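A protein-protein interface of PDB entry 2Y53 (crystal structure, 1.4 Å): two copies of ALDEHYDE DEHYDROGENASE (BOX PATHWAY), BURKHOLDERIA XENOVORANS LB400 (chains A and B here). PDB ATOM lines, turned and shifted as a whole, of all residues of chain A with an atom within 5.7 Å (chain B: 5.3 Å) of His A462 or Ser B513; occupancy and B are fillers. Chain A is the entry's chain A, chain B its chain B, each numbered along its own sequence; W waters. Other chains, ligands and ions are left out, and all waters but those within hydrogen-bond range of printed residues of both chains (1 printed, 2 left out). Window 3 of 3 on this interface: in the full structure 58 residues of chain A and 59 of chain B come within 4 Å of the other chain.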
ATOM      1  N   SER A 266      -8.456   4.908  17.103  1.00  0.00           N
ATOM      2  CA  SER A 266      -7.856   3.561  17.182  1.00  0.00           C
ATOM      3  C   SER A 266      -6.771   3.479  18.224  1.00  0.00           C
ATOM      4  O   SER A 266      -6.042   4.446  18.486  1.00  0.00           O
ATOM      5  CB  SER A 266      -7.237   3.214  15.848  1.00  0.00           C
ATOM      6  OG  SER A 266      -8.233   3.180  14.818  1.00  0.00           O
ATOM      7  N   ARG A 304     -11.835   1.636  18.685  1.00  0.00           N
ATOM      8  CA  ARG A 304     -11.475   0.445  17.894  1.00  0.00           C
ATOM      9  C   ARG A 304     -10.089   0.109  18.330  1.00  0.00           C
ATOM     10  O   ARG A 304      -9.111   0.888  18.266  1.00  0.00           O
ATOM     11  CB  ARG A 304     -11.463   0.751  16.390  1.00  0.00           C
ATOM     12  CG  ARG A 304     -12.823   1.176  15.923  1.00  0.00           C
ATOM     13  CD  ARG A 304     -12.832   1.447  14.362  1.00  0.00           C
ATOM     14  NE  ARG A 304     -11.999   2.649  14.051  1.00  0.00           N
ATOM     15  CZ  ARG A 304     -11.284   2.793  12.958  1.00  0.00           C
ATOM     16  NH1 ARG A 304     -11.301   1.896  11.935  1.00  0.00           N
ATOM     17  NH2 ARG A 304     -10.546   3.917  12.874  1.00  0.00           N
ATOM     18  N   ALA A 432      -7.240   1.295  10.578  1.00  0.00           N
ATOM     19  CA  ALA A 432      -7.422   2.585  11.248  1.00  0.00           C
ATOM     20  C   ALA A 432      -7.896   3.629  10.246  1.00  0.00           C
ATOM     21  O   ALA A 432      -8.833   4.393  10.566  1.00  0.00           O
ATOM     22  CB  ALA A 432      -6.129   3.028  11.914  1.00  0.00           C
ATOM     23  N   ARG A 433      -7.339   3.634   9.016  1.00  0.00           N
ATOM     24  CA  ARG A 433      -7.752   4.607   8.005  1.00  0.00           C
ATOM     25  C   ARG A 433      -9.214   4.384   7.626  1.00  0.00           C
ATOM     26  O   ARG A 433      -9.835   5.337   7.230  1.00  0.00           O
ATOM     27  CB  ARG A 433      -6.830   4.350   6.797  1.00  0.00           C
ATOM     28  CG  ARG A 433      -6.751   5.425   5.694  1.00  0.00           C
ATOM     29  CD  ARG A 433      -5.511   4.952   4.772  1.00  0.00           C
ATOM     30  NE  ARG A 433      -4.203   5.282   5.386  1.00  0.00           N
ATOM     31  CZ  ARG A 433      -3.066   4.635   5.176  1.00  0.00           C
ATOM     32  NH1 ARG A 433      -3.099   3.550   4.401  1.00  0.00           N
ATOM     33  NH2 ARG A 433      -1.905   5.036   5.718  1.00  0.00           N
ATOM     34  N   GLY A 437     -10.878   9.166   9.005  1.00  0.00           N
ATOM     35  CA  GLY A 437     -10.218  10.409   9.531  1.00  0.00           C
ATOM     36  C   GLY A 437     -10.586  10.546  10.994  1.00  0.00           C
ATOM     37  O   GLY A 437     -11.782  10.626  11.377  1.00  0.00           O
ATOM     38  N   SER A 438      -9.542  10.594  11.836  1.00  0.00           N
ATOM     39  CA  SER A 438      -9.759  10.562  13.300  1.00  0.00           C
ATOM     40  C   SER A 438      -8.955  11.568  14.065  1.00  0.00           C
ATOM     41  O   SER A 438      -7.911  12.086  13.541  1.00  0.00           O
ATOM     42  CB  SER A 438      -9.387   9.229  13.900  1.00  0.00           C
ATOM     43  OG  SER A 438     -10.121   8.147  13.287  1.00  0.00           O
ATOM     44  N   LEU A 439      -9.394  11.925  15.286  1.00  0.00           N
ATOM     45  CA  LEU A 439      -8.596  12.808  16.152  1.00  0.00           C
ATOM     46  C   LEU A 439      -7.262  12.164  16.538  1.00  0.00           C
ATOM     47  O   LEU A 439      -6.235  12.843  16.585  1.00  0.00           O
ATOM     48  CB  LEU A 439      -9.397  13.167  17.422  1.00  0.00           C
ATOM     49  CG  LEU A 439     -10.680  13.888  17.166  1.00  0.00           C
ATOM     50  CD1 LEU A 439     -11.485  13.940  18.434  1.00  0.00           C
ATOM     51  CD2 LEU A 439     -10.446  15.278  16.652  1.00  0.00           C
ATOM     52  N   VAL A 440      -7.294  10.902  16.896  1.00  0.00           N
ATOM     53  CA  VAL A 440      -6.115  10.284  17.523  1.00  0.00           C
ATOM     54  C   VAL A 440      -6.052   8.830  17.197  1.00  0.00           C
ATOM     55  O   VAL A 440      -7.064   8.098  17.184  1.00  0.00           O
ATOM     56  CB  VAL A 440      -6.022  10.616  19.017  1.00  0.00           C
ATOM     57  CG1 VAL A 440      -7.220  10.318  19.825  1.00  0.00           C
ATOM     58  CG2 VAL A 440      -4.729  10.061  19.701  1.00  0.00           C
ATOM     59  N   ALA A 441      -4.805   8.324  16.990  1.00  0.00           N
ATOM     60  CA  ALA A 441      -4.530   6.915  17.126  1.00  0.00           C
ATOM     61  C   ALA A 441      -3.442   6.722  18.127  1.00  0.00           C
ATOM     62  O   ALA A 441      -2.445   7.512  18.082  1.00  0.00           O
ATOM     63  CB  ALA A 441      -4.072   6.319  15.809  1.00  0.00           C
ATOM     64  N   LEU A 458       0.434   6.686  10.067  1.00  0.00           N
ATOM     65  CA  LEU A 458      -0.931   7.029  10.589  1.00  0.00           C
ATOM     66  C   LEU A 458      -1.182   8.539  10.408  1.00  0.00           C
ATOM     67  O   LEU A 458      -2.313   8.984  10.537  1.00  0.00           O
ATOM     68  CB  LEU A 458      -0.955   6.670  12.098  1.00  0.00           C
ATOM     69  CG  LEU A 458      -1.075   5.126  12.186  1.00  0.00           C
ATOM     70  CD1 LEU A 458      -0.624   4.759  13.569  1.00  0.00           C
ATOM     71  CD2 LEU A 458      -2.484   4.639  11.977  1.00  0.00           C
ATOM     72  N   ALA A 459      -0.146   9.354  10.240  1.00  0.00           N
ATOM     73  CA  ALA A 459      -0.260  10.850  10.379  1.00  0.00           C
ATOM     74  C   ALA A 459      -1.108  11.461   9.341  1.00  0.00           C
ATOM     75  O   ALA A 459      -1.613  12.574   9.651  1.00  0.00           O
ATOM     76  CB  ALA A 459       1.167  11.396  10.325  1.00  0.00           C
ATOM     77  N   ASP A 460      -1.328  10.940   8.155  1.00  0.00           N
ATOM     78  CA  ASP A 460      -2.131  11.668   7.243  1.00  0.00           C
ATOM     79  C   ASP A 460      -3.610  11.433   7.448  1.00  0.00           C
ATOM     80  O   ASP A 460      -4.458  12.120   6.829  1.00  0.00           O
ATOM     81  CB  ASP A 460      -1.737  11.387   5.760  1.00  0.00           C
ATOM     82  CG  ASP A 460      -1.988   9.967   5.357  1.00  0.00           C
ATOM     83  OD1 ASP A 460      -2.877   9.306   5.757  1.00  0.00           O
ATOM     84  OD2 ASP A 460      -1.302   9.526   4.316  1.00  0.00           O
ATOM     85  N   SER A 461      -3.972  10.542   8.359  1.00  0.00           N
ATOM     86  CA  SER A 461      -5.399  10.275   8.633  1.00  0.00           C
ATOM     87  C   SER A 461      -5.751  10.580  10.129  1.00  0.00           C
ATOM     88  O   SER A 461      -6.940  10.362  10.478  1.00  0.00           O
ATOM     89  CB  SER A 461      -5.734   8.840   8.270  1.00  0.00           C
ATOM     90  OG  SER A 461      -4.897   7.964   8.933  1.00  0.00           O
ATOM     91  N   HIS A 462      -4.795  10.975  10.943  1.00  0.00           N
ATOM     92  CA  HIS A 462      -5.040  11.191  12.386  1.00  0.00           C
ATOM     93  C   HIS A 462      -4.372  12.510  12.731  1.00  0.00           C
ATOM     94  O   HIS A 462      -3.172  12.688  12.482  1.00  0.00           O
ATOM     95  CB  HIS A 462      -4.381  10.035  13.221  1.00  0.00           C
ATOM     96  CG  HIS A 462      -5.043   8.722  12.956  1.00  0.00           C
ATOM     97  ND1 HIS A 462      -4.740   7.956  11.830  1.00  0.00           N
ATOM     98  CD2 HIS A 462      -6.040   8.073  13.609  1.00  0.00           C
ATOM     99  CE1 HIS A 462      -5.557   6.889  11.830  1.00  0.00           C
ATOM    100  NE2 HIS A 462      -6.328   6.933  12.918  1.00  0.00           N
ATOM    101  N   GLY A 463      -5.109  13.373  13.487  1.00  0.00           N
ATOM    102  CA  GLY A 463      -4.542  14.647  13.898  1.00  0.00           C
ATOM    103  C   GLY A 463      -3.483  14.523  14.993  1.00  0.00           C
ATOM    104  O   GLY A 463      -2.691  15.451  15.174  1.00  0.00           O
ATOM    105  N   ARG A 464      -3.463  13.364  15.668  1.00  0.00           N
ATOM    106  CA  ARG A 464      -2.451  13.114  16.713  1.00  0.00           C
ATOM    107  C   ARG A 464      -2.161  11.624  16.684  1.00  0.00           C
ATOM    108  O   ARG A 464      -3.078  10.826  16.609  1.00  0.00           O
ATOM    109  CB  ARG A 464      -3.002  13.564  18.075  1.00  0.00           C
ATOM    110  CG  ARG A 464      -2.003  13.396  19.275  1.00  0.00           C
ATOM    111  CD  ARG A 464      -2.363  14.329  20.442  1.00  0.00           C
ATOM    112  NE  ARG A 464      -3.752  14.132  20.933  1.00  0.00           N
ATOM    113  CZ  ARG A 464      -4.104  13.188  21.782  1.00  0.00           C
ATOM    114  NH1 ARG A 464      -3.184  12.334  22.369  1.00  0.00           N
ATOM    115  NH2 ARG A 464      -5.396  13.061  22.097  1.00  0.00           N
ATOM    116  N   VAL A 465      -0.901  11.262  16.858  1.00  0.00           N
ATOM    117  CA  VAL A 465      -0.478   9.847  16.964  1.00  0.00           C
ATOM    118  C   VAL A 465       0.289   9.753  18.275  1.00  0.00           C
ATOM    119  O   VAL A 465       1.229  10.524  18.463  1.00  0.00           O
ATOM    120  CB  VAL A 465       0.400   9.370  15.781  1.00  0.00           C
ATOM    121  CG1 VAL A 465       0.681   7.876  15.975  1.00  0.00           C
ATOM    122  CG2 VAL A 465      -0.345   9.602  14.440  1.00  0.00           C
ATOM    123  N   LEU A 487      -1.402  19.729  18.722  1.00  0.00           N
ATOM    124  CA  LEU A 487      -2.601  19.902  17.906  1.00  0.00           C
ATOM    125  C   LEU A 487      -3.724  19.022  18.361  1.00  0.00           C
ATOM    126  O   LEU A 487      -3.529  17.841  18.711  1.00  0.00           O
ATOM    127  CB  LEU A 487      -2.266  19.506  16.457  1.00  0.00           C
ATOM    128  CG  LEU A 487      -3.326  19.798  15.391  1.00  0.00           C
ATOM    129  CD1 LEU A 487      -3.335  21.292  15.240  1.00  0.00           C
ATOM    130  CD2 LEU A 487      -2.952  19.088  14.039  1.00  0.00           C
ATOM    131  N   GLY A 489      -7.550  17.877  16.757  1.00  0.00           N
ATOM    132  CA  GLY A 489      -8.348  17.988  15.503  1.00  0.00           C
ATOM    133  C   GLY A 489      -8.049  16.785  14.677  1.00  0.00           C
ATOM    134  O   GLY A 489      -7.203  15.959  14.966  1.00  0.00           O
ATOM    135  N   GLY A 490      -8.705  16.688  13.565  1.00  0.00           N
ATOM    136  CA  GLY A 490      -8.404  15.592  12.635  1.00  0.00           C
ATOM    137  C   GLY A 490      -9.160  15.771  11.329  1.00  0.00           C
ATOM    138  O   GLY A 490     -10.137  16.497  11.283  1.00  0.00           O
ATOM    139  N   PRO A 491      -8.660  15.096  10.289  1.00  0.00           N
ATOM    140  CA  PRO A 491      -9.301  15.187   8.975  1.00  0.00           C
ATOM    141  C   PRO A 491     -10.571  14.373   8.882  1.00  0.00           C
ATOM    142  O   PRO A 491     -10.932  13.538   9.744  1.00  0.00           O
ATOM    143  CB  PRO A 491      -8.223  14.665   8.020  1.00  0.00           C
ATOM    144  CG  PRO A 491      -7.519  13.534   8.846  1.00  0.00           C
ATOM    145  CD  PRO A 491      -7.520  14.128  10.324  1.00  0.00           C
ATOM    146  N   GLN B 145       6.474  16.087  18.310  1.00  0.00           N
ATOM    147  CA  GLN B 145       6.914  16.738  17.096  1.00  0.00           C
ATOM    148  C   GLN B 145       5.694  16.793  16.165  1.00  0.00           C
ATOM    149  O   GLN B 145       5.106  15.720  15.864  1.00  0.00           O
ATOM    150  CB  GLN B 145       8.050  15.884  16.413  1.00  0.00           C
ATOM    151  CG  GLN B 145       8.447  16.343  14.990  1.00  0.00           C
ATOM    152  CD  GLN B 145       9.120  17.734  15.022  1.00  0.00           C
ATOM    153  OE1 GLN B 145      10.206  17.884  15.613  1.00  0.00           O
ATOM    154  NE2 GLN B 145       8.510  18.736  14.391  1.00  0.00           N
ATOM    155  N   HIS B 146       5.396  17.932  15.619  1.00  0.00           N
ATOM    156  CA  HIS B 146       4.369  18.002  14.582  1.00  0.00           C
ATOM    157  C   HIS B 146       4.932  17.747  13.201  1.00  0.00           C
ATOM    158  O   HIS B 146       6.096  18.134  12.882  1.00  0.00           O
ATOM    159  CB  HIS B 146       3.713  19.376  14.576  1.00  0.00           C
ATOM    160  CG  HIS B 146       2.884  19.653  15.826  1.00  0.00           C
ATOM    161  ND1 HIS B 146       3.436  19.946  17.072  1.00  0.00           N
ATOM    162  CD2 HIS B 146       1.525  19.630  16.019  1.00  0.00           C
ATOM    163  CE1 HIS B 146       2.464  20.158  17.943  1.00  0.00           C
ATOM    164  NE2 HIS B 146       1.301  19.921  17.363  1.00  0.00           N
ATOM    165  N   VAL B 147       4.163  17.084  12.346  1.00  0.00           N
ATOM    166  CA  VAL B 147       4.573  16.767  10.990  1.00  0.00           C
ATOM    167  C   VAL B 147       3.462  17.173  10.002  1.00  0.00           C
ATOM    168  O   VAL B 147       2.264  17.307  10.381  1.00  0.00           O
ATOM    169  CB  VAL B 147       4.903  15.302  10.839  1.00  0.00           C
ATOM    170  CG1 VAL B 147       6.100  14.903  11.723  1.00  0.00           C
ATOM    171  CG2 VAL B 147       3.746  14.355  11.083  1.00  0.00           C
ATOM    172  N   LEU B 148       3.839  17.363   8.755  1.00  0.00           N
ATOM    173  CA  LEU B 148       2.918  17.606   7.615  1.00  0.00           C
ATOM    174  C   LEU B 148       3.084  16.477   6.655  1.00  0.00           C
ATOM    175  O   LEU B 148       4.207  16.178   6.237  1.00  0.00           O
ATOM    176  CB  LEU B 148       3.319  18.925   6.897  1.00  0.00           C
ATOM    177  CG  LEU B 148       3.224  20.152   7.794  1.00  0.00           C
ATOM    178  CD1 LEU B 148       3.872  21.419   7.233  1.00  0.00           C
ATOM    179  CD2 LEU B 148       1.841  20.446   8.112  1.00  0.00           C
ATOM    180  N   ARG B 511      -1.882  17.391   5.541  1.00  0.00           N
ATOM    181  CA  ARG B 511      -2.496  17.296   6.866  1.00  0.00           C
ATOM    182  C   ARG B 511      -1.417  17.374   7.931  1.00  0.00           C
ATOM    183  O   ARG B 511      -0.403  16.670   7.844  1.00  0.00           O
ATOM    184  CB  ARG B 511      -3.343  16.037   7.127  1.00  0.00           C
ATOM    185  CG  ARG B 511      -3.821  15.983   8.621  1.00  0.00           C
ATOM    186  CD  ARG B 511      -5.266  16.590   8.975  1.00  0.00           C
ATOM    187  NE  ARG B 511      -5.182  17.082  10.408  1.00  0.00           N
ATOM    188  CZ  ARG B 511      -4.728  18.282  10.819  1.00  0.00           C
ATOM    189  NH1 ARG B 511      -4.283  19.167   9.985  1.00  0.00           N
ATOM    190  NH2 ARG B 511      -4.838  18.544  12.098  1.00  0.00           N
ATOM    191  N   ARG B 512      -1.709  18.155   8.942  1.00  0.00           N
ATOM    192  CA  ARG B 512      -0.815  18.326  10.069  1.00  0.00           C
ATOM    193  C   ARG B 512      -1.145  17.340  11.175  1.00  0.00           C
ATOM    194  O   ARG B 512      -2.353  17.069  11.469  1.00  0.00           O
ATOM    195  CB  ARG B 512      -1.014  19.696  10.636  1.00  0.00           C
ATOM    196  CG  ARG B 512       0.019  20.093  11.673  1.00  0.00           C
ATOM    197  CD  ARG B 512      -0.323  21.396  12.377  1.00  0.00           C
ATOM    198  NE  ARG B 512      -0.793  22.432  11.473  1.00  0.00           N
ATOM    199  CZ  ARG B 512      -0.024  23.174  10.715  1.00  0.00           C
ATOM    200  NH1 ARG B 512       1.278  23.062  10.780  1.00  0.00           N
ATOM    201  NH2 ARG B 512      -0.571  24.085   9.917  1.00  0.00           N
ATOM    202  N   SER B 513      -0.165  16.751  11.854  1.00  0.00           N
ATOM    203  CA  SER B 513      -0.412  15.779  12.953  1.00  0.00           C
ATOM    204  C   SER B 513       0.587  16.034  14.066  1.00  0.00           C
ATOM    205  O   SER B 513       1.812  16.252  13.795  1.00  0.00           O
ATOM    206  CB  SER B 513      -0.200  14.329  12.529  1.00  0.00           C
ATOM    207  OG  SER B 513      -0.981  14.181  11.424  1.00  0.00           O
ATOM    208  N   ALA B 514       0.169  15.922  15.330  1.00  0.00           N
ATOM    209  CA  ALA B 514       1.076  15.908  16.491  1.00  0.00           C
ATOM    210  C   ALA B 514       1.502  14.483  16.750  1.00  0.00           C
ATOM    211  O   ALA B 514       0.643  13.680  17.105  1.00  0.00           O
ATOM    212  CB  ALA B 514       0.383  16.502  17.696  1.00  0.00           C
ATOM    213  N   ILE B 515       2.778  14.184  16.703  1.00  0.00           N
ATOM    214  CA  ILE B 515       3.251  12.867  17.110  1.00  0.00           C
ATOM    215  C   ILE B 515       3.843  12.930  18.503  1.00  0.00           C
ATOM    216  O   ILE B 515       4.763  13.754  18.765  1.00  0.00           O
ATOM    217  CB  ILE B 515       4.359  12.345  16.146  1.00  0.00           C
ATOM    218  CG1 ILE B 515       3.964  12.552  14.689  1.00  0.00           C
ATOM    219  CG2 ILE B 515       4.780  10.917  16.533  1.00  0.00           C
ATOM    220  CD1 ILE B 515       2.795  11.916  14.305  1.00  0.00           C
HETATM  221  O   HOH W   1       0.633  14.432   9.086  1.00  0.00           O
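Of the 21 printed residues of chain A, 7 touch a printed residue of chain B.
Of the 9 printed residues of chain B, 7 touch a printed residue of chain A.
Among the printed residues, 13 pairs touch across the chains.
Water W1 lies within hydrogen-bond range of the backbone carbonyl oxygen of Arg B511 (2.8 Å), the side-chain hydroxyl of Ser B513 (2.9 Å) and the backbone carbonyl oxygen of Ala A459 (3.0 Å).
O of Gly A463 is in hydrogen-bond range of N of Ala B514 (2.9 Å).
The backbone NH (N) of Val A465 is in hydrogen-bond range of the backbone carbonyl oxygen (O) of Ala B514 (2.9 Å).
The backbone NH (N) of Leu A487 lies within hydrogen-bond range of a ring nitrogen (NE2) of His B146 (3.0 Å).
The backbone carbonyl oxygen (O) of Ala A459 lies within hydrogen-bond range of the side-chain hydroxyl (OG) of Ser B513 (2.5 Å).
The backbone carbonyl oxygen (O) of His A462 is in hydrogen-bond range of the side-chain hydroxyl (OG) of Ser B513 (2.9 Å).
Arg A304 touches none of the printed residues of chain B.
Of the printed residues of chain B, Gly A463 touches Ser B513 and Ala B514.
Of the printed residues of chain B, Arg A464 touches Ala B514 (3.2 Å).
Of the printed residues of chain B, Val A465 touches Ala B514 (2.9 Å) and Ile B515 (3.4 Å).
Of the printed residues of chain A, Val B147 touches Ala A459.
Printed residues of chain A within 4 Å of Arg B511: Leu A487 (2.8 Å) and Pro A491 (3.6 Å).
Ser B513 touches just these residues of chain A: Ala A459, His A462 and Gly A463.
The nearest residue of chain A that does not touch Ser B513 is Leu A487 (4.2 Å).
The nearest printed residue of chain B that does not touch Pro A491 is Arg B512 (6.1 Å).
No position is printed for both chains.
Of the 13 pairs that touch across the chains among the printed residues, none has its exchanged pair printed and touching as well.
The backbone carbonyl oxygen (O) of Ser A438 is in hydrogen-bond range of the backbone NH (N) of Gly A463 (3.1 Å).
O of Leu A439 is in hydrogen-bond range of N of Arg A464 (3.0 Å).
O of Arg A464 is in hydrogen-bond range of N of Ala A441 (3.1 Å).
The side-chain hydroxyl (OG) of Ser A461 is in hydrogen-bond range of a ring nitrogen (ND1) of His A462 (2.9 Å).
The backbone NH of Val B147 is in hydrogen-bond range of the backbone carbonyl oxygen of Ser B513 (2.9 Å).
A ring nitrogen (ND1) of His A462 lies within hydrogen-bond range of the backbone carbonyl oxygen (O) of Leu A458, at 2.9 Å.
Among the printed residues, merely in contact across the chains: Ala A459 with Val B147 (3.998 Å), Gly A463 with Ser B513 (3.2 Å), Arg A464 with Ala B514 (3.2 Å), Val A465 with Ile B515 (3.4 Å), Leu A487 with Arg B511 (2.8 Å), Leu A487 with Arg B512 (3.3 Å), Leu A487 with Ala B514 (3.8 Å) and Pro A491 with Arg B511 (3.6 Å).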
